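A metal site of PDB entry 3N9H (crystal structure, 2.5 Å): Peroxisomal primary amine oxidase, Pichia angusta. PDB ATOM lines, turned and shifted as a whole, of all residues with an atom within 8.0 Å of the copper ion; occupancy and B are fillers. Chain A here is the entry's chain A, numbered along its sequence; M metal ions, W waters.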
ATOM      1  N   VAL A 303      -4.740 -28.249 -25.934  1.00  0.00           N
ATOM      2  CA  VAL A 303      -4.152 -28.091 -24.604  1.00  0.00           C
ATOM      3  C   VAL A 303      -4.899 -29.042 -23.666  1.00  0.00           C
ATOM      4  O   VAL A 303      -5.807 -28.641 -22.934  1.00  0.00           O
ATOM      5  CB  VAL A 303      -4.315 -26.608 -24.166  1.00  0.00           C
ATOM      6  CG1 VAL A 303      -3.623 -26.343 -22.849  1.00  0.00           C
ATOM      7  CG2 VAL A 303      -3.740 -25.704 -25.246  1.00  0.00           C
ATOM      8  N   ASN A 404      -7.511 -17.387 -20.097  1.00  0.00           N
ATOM      9  CA  ASN A 404      -6.445 -17.197 -19.136  1.00  0.00           C
ATOM     10  C   ASN A 404      -5.024 -17.150 -19.690  1.00  0.00           C
ATOM     11  O   ASN A 404      -4.178 -16.492 -19.104  1.00  0.00           O
ATOM     12  CB  ASN A 404      -6.530 -18.257 -18.053  1.00  0.00           C
ATOM     13  CG  ASN A 404      -6.530 -19.653 -18.621  1.00  0.00           C
ATOM     14  OD1 ASN A 404      -7.399 -20.014 -19.416  1.00  0.00           O
ATOM     15  ND2 ASN A 404      -5.538 -20.455 -18.224  1.00  0.00           N
ATOM     16  N   TPQ A 405      -4.733 -17.834 -20.793  1.00  0.00           N
ATOM     17  CA  TPQ A 405      -3.369 -17.815 -21.317  1.00  0.00           C
ATOM     18  CB  TPQ A 405      -2.693 -19.160 -21.648  1.00  0.00           C
ATOM     19  C   TPQ A 405      -3.102 -16.989 -22.541  1.00  0.00           C
ATOM     20  O   TPQ A 405      -3.997 -16.746 -23.343  1.00  0.00           O
ATOM     21  C1  TPQ A 405      -3.420 -20.413 -21.364  1.00  0.00           C
ATOM     22  C2  TPQ A 405      -2.826 -21.381 -20.517  1.00  0.00           C
ATOM     23  O2  TPQ A 405      -1.718 -21.145 -20.049  1.00  0.00           O
ATOM     24  C3  TPQ A 405      -3.501 -22.584 -20.214  1.00  0.00           C
ATOM     25  C4  TPQ A 405      -4.798 -22.834 -20.767  1.00  0.00           C
ATOM     26  O4  TPQ A 405      -5.424 -24.028 -20.433  1.00  0.00           O
ATOM     27  C5  TPQ A 405      -5.412 -21.862 -21.644  1.00  0.00           C
ATOM     28  O5  TPQ A 405      -6.609 -22.044 -22.178  1.00  0.00           O
ATOM     29  C6  TPQ A 405      -4.708 -20.653 -21.927  1.00  0.00           C
ATOM     30  N   TYR A 407      -0.405 -16.561 -25.828  1.00  0.00           N
ATOM     31  CA  TYR A 407       0.551 -17.245 -26.672  1.00  0.00           C
ATOM     32  C   TYR A 407       1.248 -16.185 -27.517  1.00  0.00           C
ATOM     33  O   TYR A 407       0.605 -15.431 -28.252  1.00  0.00           O
ATOM     34  CB  TYR A 407      -0.164 -18.249 -27.584  1.00  0.00           C
ATOM     35  CG  TYR A 407      -0.762 -19.412 -26.850  1.00  0.00           C
ATOM     36  CD1 TYR A 407      -2.056 -19.361 -26.349  1.00  0.00           C
ATOM     37  CD2 TYR A 407      -0.005 -20.566 -26.619  1.00  0.00           C
ATOM     38  CE1 TYR A 407      -2.597 -20.435 -25.628  1.00  0.00           C
ATOM     39  CE2 TYR A 407      -0.517 -21.635 -25.899  1.00  0.00           C
ATOM     40  CZ  TYR A 407      -1.813 -21.565 -25.408  1.00  0.00           C
ATOM     41  OH  TYR A 407      -2.317 -22.623 -24.688  1.00  0.00           O
ATOM     42  N   LEU A 425       4.965 -19.021 -23.955  1.00  0.00           N
ATOM     43  CA  LEU A 425       3.711 -19.183 -23.230  1.00  0.00           C
ATOM     44  C   LEU A 425       3.770 -18.294 -22.018  1.00  0.00           C
ATOM     45  O   LEU A 425       4.785 -18.270 -21.299  1.00  0.00           O
ATOM     46  CB  LEU A 425       3.513 -20.603 -22.739  1.00  0.00           C
ATOM     47  CG  LEU A 425       3.618 -21.784 -23.698  1.00  0.00           C
ATOM     48  CD1 LEU A 425       3.128 -23.053 -22.985  1.00  0.00           C
ATOM     49  CD2 LEU A 425       2.790 -21.528 -24.949  1.00  0.00           C
ATOM     50  N   THR A 426       2.711 -17.524 -21.804  1.00  0.00           N
ATOM     51  CA  THR A 426       2.656 -16.677 -20.633  1.00  0.00           C
ATOM     52  C   THR A 426       1.191 -16.550 -20.271  1.00  0.00           C
ATOM     53  O   THR A 426       0.363 -17.340 -20.739  1.00  0.00           O
ATOM     54  CB  THR A 426       3.314 -15.312 -20.906  1.00  0.00           C
ATOM     55  OG1 THR A 426       3.430 -14.596 -19.673  1.00  0.00           O
ATOM     56  CG2 THR A 426       2.487 -14.513 -21.900  1.00  0.00           C
ATOM     57  N   ILE A 428      -1.979 -16.691 -17.506  1.00  0.00           N
ATOM     58  CA  ILE A 428      -2.329 -17.252 -16.220  1.00  0.00           C
ATOM     59  C   ILE A 428      -2.732 -18.719 -16.264  1.00  0.00           C
ATOM     60  O   ILE A 428      -3.371 -19.175 -17.217  1.00  0.00           O
ATOM     61  CB  ILE A 428      -3.450 -16.386 -15.612  1.00  0.00           C
ATOM     62  CG1 ILE A 428      -2.932 -14.947 -15.483  1.00  0.00           C
ATOM     63  CG2 ILE A 428      -3.921 -16.962 -14.268  1.00  0.00           C
ATOM     64  CD1 ILE A 428      -3.971 -13.934 -15.162  1.00  0.00           C
ATOM     65  N   LEU A 429      -2.350 -19.464 -15.227  1.00  0.00           N
ATOM     66  CA  LEU A 429      -2.652 -20.885 -15.130  1.00  0.00           C
ATOM     67  C   LEU A 429      -4.142 -21.130 -15.118  1.00  0.00           C
ATOM     68  O   LEU A 429      -4.906 -20.343 -14.565  1.00  0.00           O
ATOM     69  CB  LEU A 429      -2.091 -21.444 -13.838  1.00  0.00           C
ATOM     70  CG  LEU A 429      -0.582 -21.523 -13.721  1.00  0.00           C
ATOM     71  CD1 LEU A 429      -0.196 -21.887 -12.285  1.00  0.00           C
ATOM     72  CD2 LEU A 429      -0.053 -22.559 -14.726  1.00  0.00           C
ATOM     73  N   ASN A 430      -4.586 -22.214 -15.747  1.00  0.00           N
ATOM     74  CA  ASN A 430      -5.991 -22.555 -15.696  1.00  0.00           C
ATOM     75  C   ASN A 430      -6.100 -23.120 -14.272  1.00  0.00           C
ATOM     76  O   ASN A 430      -5.426 -24.087 -13.935  1.00  0.00           O
ATOM     77  CB  ASN A 430      -6.326 -23.638 -16.723  1.00  0.00           C
ATOM     78  CG  ASN A 430      -7.599 -24.395 -16.383  1.00  0.00           C
ATOM     79  OD1 ASN A 430      -7.616 -25.625 -16.381  1.00  0.00           O
ATOM     80  ND2 ASN A 430      -8.673 -23.664 -16.097  1.00  0.00           N
ATOM     81  N   HIS A 454      -4.106 -27.630 -12.644  1.00  0.00           N
ATOM     82  CA  HIS A 454      -3.952 -28.972 -13.221  1.00  0.00           C
ATOM     83  C   HIS A 454      -2.827 -29.113 -14.233  1.00  0.00           C
ATOM     84  O   HIS A 454      -2.481 -28.149 -14.922  1.00  0.00           O
ATOM     85  CB  HIS A 454      -5.251 -29.384 -13.904  1.00  0.00           C
ATOM     86  CG  HIS A 454      -6.382 -29.644 -12.959  1.00  0.00           C
ATOM     87  ND1 HIS A 454      -7.704 -29.439 -13.309  1.00  0.00           N
ATOM     88  CD2 HIS A 454      -6.399 -30.133 -11.697  1.00  0.00           C
ATOM     89  CE1 HIS A 454      -8.476 -29.801 -12.307  1.00  0.00           C
ATOM     90  NE2 HIS A 454      -7.708 -30.224 -11.318  1.00  0.00           N
ATOM     91  N   ASN A 455      -2.251 -30.305 -14.315  1.00  0.00           N
ATOM     92  CA  ASN A 455      -1.206 -30.579 -15.302  1.00  0.00           C
ATOM     93  C   ASN A 455      -1.885 -30.480 -16.670  1.00  0.00           C
ATOM     94  O   ASN A 455      -3.087 -30.740 -16.809  1.00  0.00           O
ATOM     95  CB  ASN A 455      -0.668 -32.006 -15.161  1.00  0.00           C
ATOM     96  CG  ASN A 455      -0.132 -32.291 -13.796  1.00  0.00           C
ATOM     97  OD1 ASN A 455       0.287 -31.377 -13.077  1.00  0.00           O
ATOM     98  ND2 ASN A 455      -0.107 -33.571 -13.418  1.00  0.00           N
ATOM     99  N   HIS A 456      -1.132 -30.123 -17.702  1.00  0.00           N
ATOM    100  CA  HIS A 456      -1.717 -30.047 -19.036  1.00  0.00           C
ATOM    101  C   HIS A 456      -0.579 -29.952 -20.032  1.00  0.00           C
ATOM    102  O   HIS A 456       0.541 -29.589 -19.661  1.00  0.00           O
ATOM    103  CB  HIS A 456      -2.610 -28.816 -19.155  1.00  0.00           C
ATOM    104  CG  HIS A 456      -1.888 -27.536 -18.840  1.00  0.00           C
ATOM    105  ND1 HIS A 456      -1.608 -27.155 -17.542  1.00  0.00           N
ATOM    106  CD2 HIS A 456      -1.288 -26.630 -19.639  1.00  0.00           C
ATOM    107  CE1 HIS A 456      -0.860 -26.064 -17.566  1.00  0.00           C
ATOM    108  NE2 HIS A 456      -0.658 -25.717 -18.824  1.00  0.00           N
ATOM    109  N   GLN A 457      -0.856 -30.289 -21.282  1.00  0.00           N
ATOM    110  CA  GLN A 457       0.156 -30.165 -22.323  1.00  0.00           C
ATOM    111  C   GLN A 457      -0.319 -29.042 -23.256  1.00  0.00           C
ATOM    112  O   GLN A 457      -1.505 -28.715 -23.289  1.00  0.00           O
ATOM    113  CB  GLN A 457       0.296 -31.455 -23.154  1.00  0.00           C
ATOM    114  CG  GLN A 457       0.431 -32.775 -22.400  1.00  0.00           C
ATOM    115  CD  GLN A 457       0.787 -33.945 -23.332  1.00  0.00           C
ATOM    116  OE1 GLN A 457       1.952 -34.166 -23.637  1.00  0.00           O
ATOM    117  NE2 GLN A 457      -0.221 -34.682 -23.798  1.00  0.00           N
ATOM    118  N   HIS A 458       0.624 -28.454 -23.996  1.00  0.00           N
ATOM    119  CA  HIS A 458       0.326 -27.419 -24.988  1.00  0.00           C
ATOM    120  C   HIS A 458       0.882 -28.022 -26.279  1.00  0.00           C
ATOM    121  O   HIS A 458       2.103 -28.104 -26.450  1.00  0.00           O
ATOM    122  CB  HIS A 458       1.066 -26.126 -24.683  1.00  0.00           C
ATOM    123  CG  HIS A 458       0.554 -25.399 -23.489  1.00  0.00           C
ATOM    124  ND1 HIS A 458      -0.491 -24.494 -23.562  1.00  0.00           N
ATOM    125  CD2 HIS A 458       0.920 -25.440 -22.183  1.00  0.00           C
ATOM    126  CE1 HIS A 458      -0.732 -24.008 -22.355  1.00  0.00           C
ATOM    127  NE2 HIS A 458       0.111 -24.571 -21.506  1.00  0.00           N
ATOM    128  N   ILE A 622       4.815 -28.413 -25.302  1.00  0.00           N
ATOM    129  CA  ILE A 622       5.405 -28.775 -24.021  1.00  0.00           C
ATOM    130  C   ILE A 622       4.399 -29.432 -23.089  1.00  0.00           C
ATOM    131  O   ILE A 622       3.194 -29.406 -23.345  1.00  0.00           O
ATOM    132  CB  ILE A 622       5.994 -27.531 -23.317  1.00  0.00           C
ATOM    133  CG1 ILE A 622       4.930 -26.462 -23.161  1.00  0.00           C
ATOM    134  CG2 ILE A 622       7.143 -26.956 -24.131  1.00  0.00           C
ATOM    135  CD1 ILE A 622       4.593 -26.171 -21.745  1.00  0.00           C
ATOM    136  N   THR A 623       4.915 -30.065 -22.044  1.00  0.00           N
ATOM    137  CA  THR A 623       4.065 -30.693 -21.038  1.00  0.00           C
ATOM    138  C   THR A 623       4.279 -29.829 -19.801  1.00  0.00           C
ATOM    139  O   THR A 623       5.399 -29.671 -19.318  1.00  0.00           O
ATOM    140  CB  THR A 623       4.493 -32.141 -20.799  1.00  0.00           C
ATOM    141  OG1 THR A 623       4.240 -32.887 -21.995  1.00  0.00           O
ATOM    142  CG2 THR A 623       3.700 -32.762 -19.672  1.00  0.00           C
ATOM    143  N   HIS A 624       3.197 -29.267 -19.294  1.00  0.00           N
ATOM    144  CA  HIS A 624       3.294 -28.357 -18.163  1.00  0.00           C
ATOM    145  C   HIS A 624       2.797 -28.888 -16.823  1.00  0.00           C
ATOM    146  O   HIS A 624       1.622 -29.225 -16.665  1.00  0.00           O
ATOM    147  CB  HIS A 624       2.540 -27.071 -18.542  1.00  0.00           C
ATOM    148  CG  HIS A 624       2.746 -25.932 -17.592  1.00  0.00           C
ATOM    149  ND1 HIS A 624       2.177 -24.695 -17.782  1.00  0.00           N
ATOM    150  CD2 HIS A 624       3.458 -25.837 -16.445  1.00  0.00           C
ATOM    151  CE1 HIS A 624       2.526 -23.887 -16.798  1.00  0.00           C
ATOM    152  NE2 HIS A 624       3.297 -24.564 -15.965  1.00  0.00           N
ATOM    153  N   PHE A 625       3.723 -28.964 -15.870  1.00  0.00           N
ATOM    154  CA  PHE A 625       3.430 -29.388 -14.490  1.00  0.00           C
ATOM    155  C   PHE A 625       3.635 -28.099 -13.709  1.00  0.00           C
ATOM    156  O   PHE A 625       4.766 -27.736 -13.378  1.00  0.00           O
ATOM    157  CB  PHE A 625       4.422 -30.460 -14.027  1.00  0.00           C
ATOM    158  CG  PHE A 625       4.300 -31.765 -14.774  1.00  0.00           C
ATOM    159  CD1 PHE A 625       3.193 -32.596 -14.575  1.00  0.00           C
ATOM    160  CD2 PHE A 625       5.270 -32.148 -15.706  1.00  0.00           C
ATOM    161  CE1 PHE A 625       3.054 -33.800 -15.289  1.00  0.00           C
ATOM    162  CE2 PHE A 625       5.139 -33.341 -16.420  1.00  0.00           C
ATOM    163  CZ  PHE A 625       4.032 -34.172 -16.211  1.00  0.00           C
ATOM    164  N   PRO A 626       2.542 -27.371 -13.433  1.00  0.00           N
ATOM    165  CA  PRO A 626       2.589 -26.099 -12.706  1.00  0.00           C
ATOM    166  C   PRO A 626       3.394 -26.093 -11.421  1.00  0.00           C
ATOM    167  O   PRO A 626       3.447 -27.082 -10.689  1.00  0.00           O
ATOM    168  CB  PRO A 626       1.117 -25.788 -12.445  1.00  0.00           C
ATOM    169  CG  PRO A 626       0.395 -26.532 -13.564  1.00  0.00           C
ATOM    170  CD  PRO A 626       1.149 -27.826 -13.616  1.00  0.00           C
ATOM    171  N   ASP A 630       4.790 -20.107 -11.378  1.00  0.00           N
ATOM    172  CA  ASP A 630       3.893 -19.813 -12.483  1.00  0.00           C
ATOM    173  C   ASP A 630       2.706 -18.958 -12.047  1.00  0.00           C
ATOM    174  O   ASP A 630       1.910 -18.509 -12.888  1.00  0.00           O
ATOM    175  CB  ASP A 630       3.331 -21.108 -13.103  1.00  0.00           C
ATOM    176  CG  ASP A 630       4.405 -22.067 -13.617  1.00  0.00           C
ATOM    177  OD1 ASP A 630       5.446 -21.611 -14.136  1.00  0.00           O
ATOM    178  OD2 ASP A 630       4.194 -23.292 -13.540  1.00  0.00           O
ATOM    179  N   MET A 634       2.376 -16.096 -15.013  1.00  0.00           N
ATOM    180  CA  MET A 634       3.579 -16.876 -15.263  1.00  0.00           C
ATOM    181  C   MET A 634       4.620 -16.306 -16.210  1.00  0.00           C
ATOM    182  O   MET A 634       4.306 -15.679 -17.219  1.00  0.00           O
ATOM    183  CB  MET A 634       3.224 -18.280 -15.721  1.00  0.00           C
ATOM    184  CG  MET A 634       3.033 -18.436 -17.200  1.00  0.00           C
ATOM    185  SD  MET A 634       2.591 -20.125 -17.623  1.00  0.00           S
ATOM    186  CE  MET A 634       0.733 -19.952 -17.766  1.00  0.00           C
ATOM    187  N   GLU A 637       7.453 -19.082 -21.085  1.00  0.00           N
ATOM    188  CA  GLU A 637       8.107 -20.371 -21.270  1.00  0.00           C
ATOM    189  C   GLU A 637       8.276 -20.492 -22.782  1.00  0.00           C
ATOM    190  O   GLU A 637       7.302 -20.390 -23.537  1.00  0.00           O
ATOM    191  CB  GLU A 637       7.291 -21.542 -20.762  1.00  0.00           C
ATOM    192  CG  GLU A 637       8.201 -22.751 -20.654  1.00  0.00           C
ATOM    193  CD  GLU A 637       7.497 -24.036 -20.287  1.00  0.00           C
ATOM    194  OE1 GLU A 637       6.362 -23.967 -19.752  1.00  0.00           O
ATOM    195  OE2 GLU A 637       8.098 -25.112 -20.516  1.00  0.00           O
HETATM  196 CU    CU M   1       0.878 -24.350 -19.473  1.00  0.00          CU
HETATM  197  O   HOH W   1      -0.974 -22.576 -18.409  1.00  0.00           O
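ND1 of His 456 is in hydrogen-bond range of O of His 454, at 2.9 Å. OD2 of Asp 630 sits at hydrogen-bond distance from NE2 of His 624. N of His 458 sits at hydrogen-bond distance from O of Ile 622 (2.8 Å). A ring nitrogen (ND1) of His 458 is in hydrogen-bond range of the side-chain hydroxyl of Tyr 407, 2.8 Å away.
Of the 22 residues printed, 3 come within 4 Å of the copper ion.
The copper ion is bound by a ring nitrogen (NE2) of His 456, a ring nitrogen (ND1) of His 624 and a ring nitrogen (NE2) of His 458. The copper ion has three donor atoms within binding distance. Slightly farther from the copper ion lies water W1 (2.8 Å).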
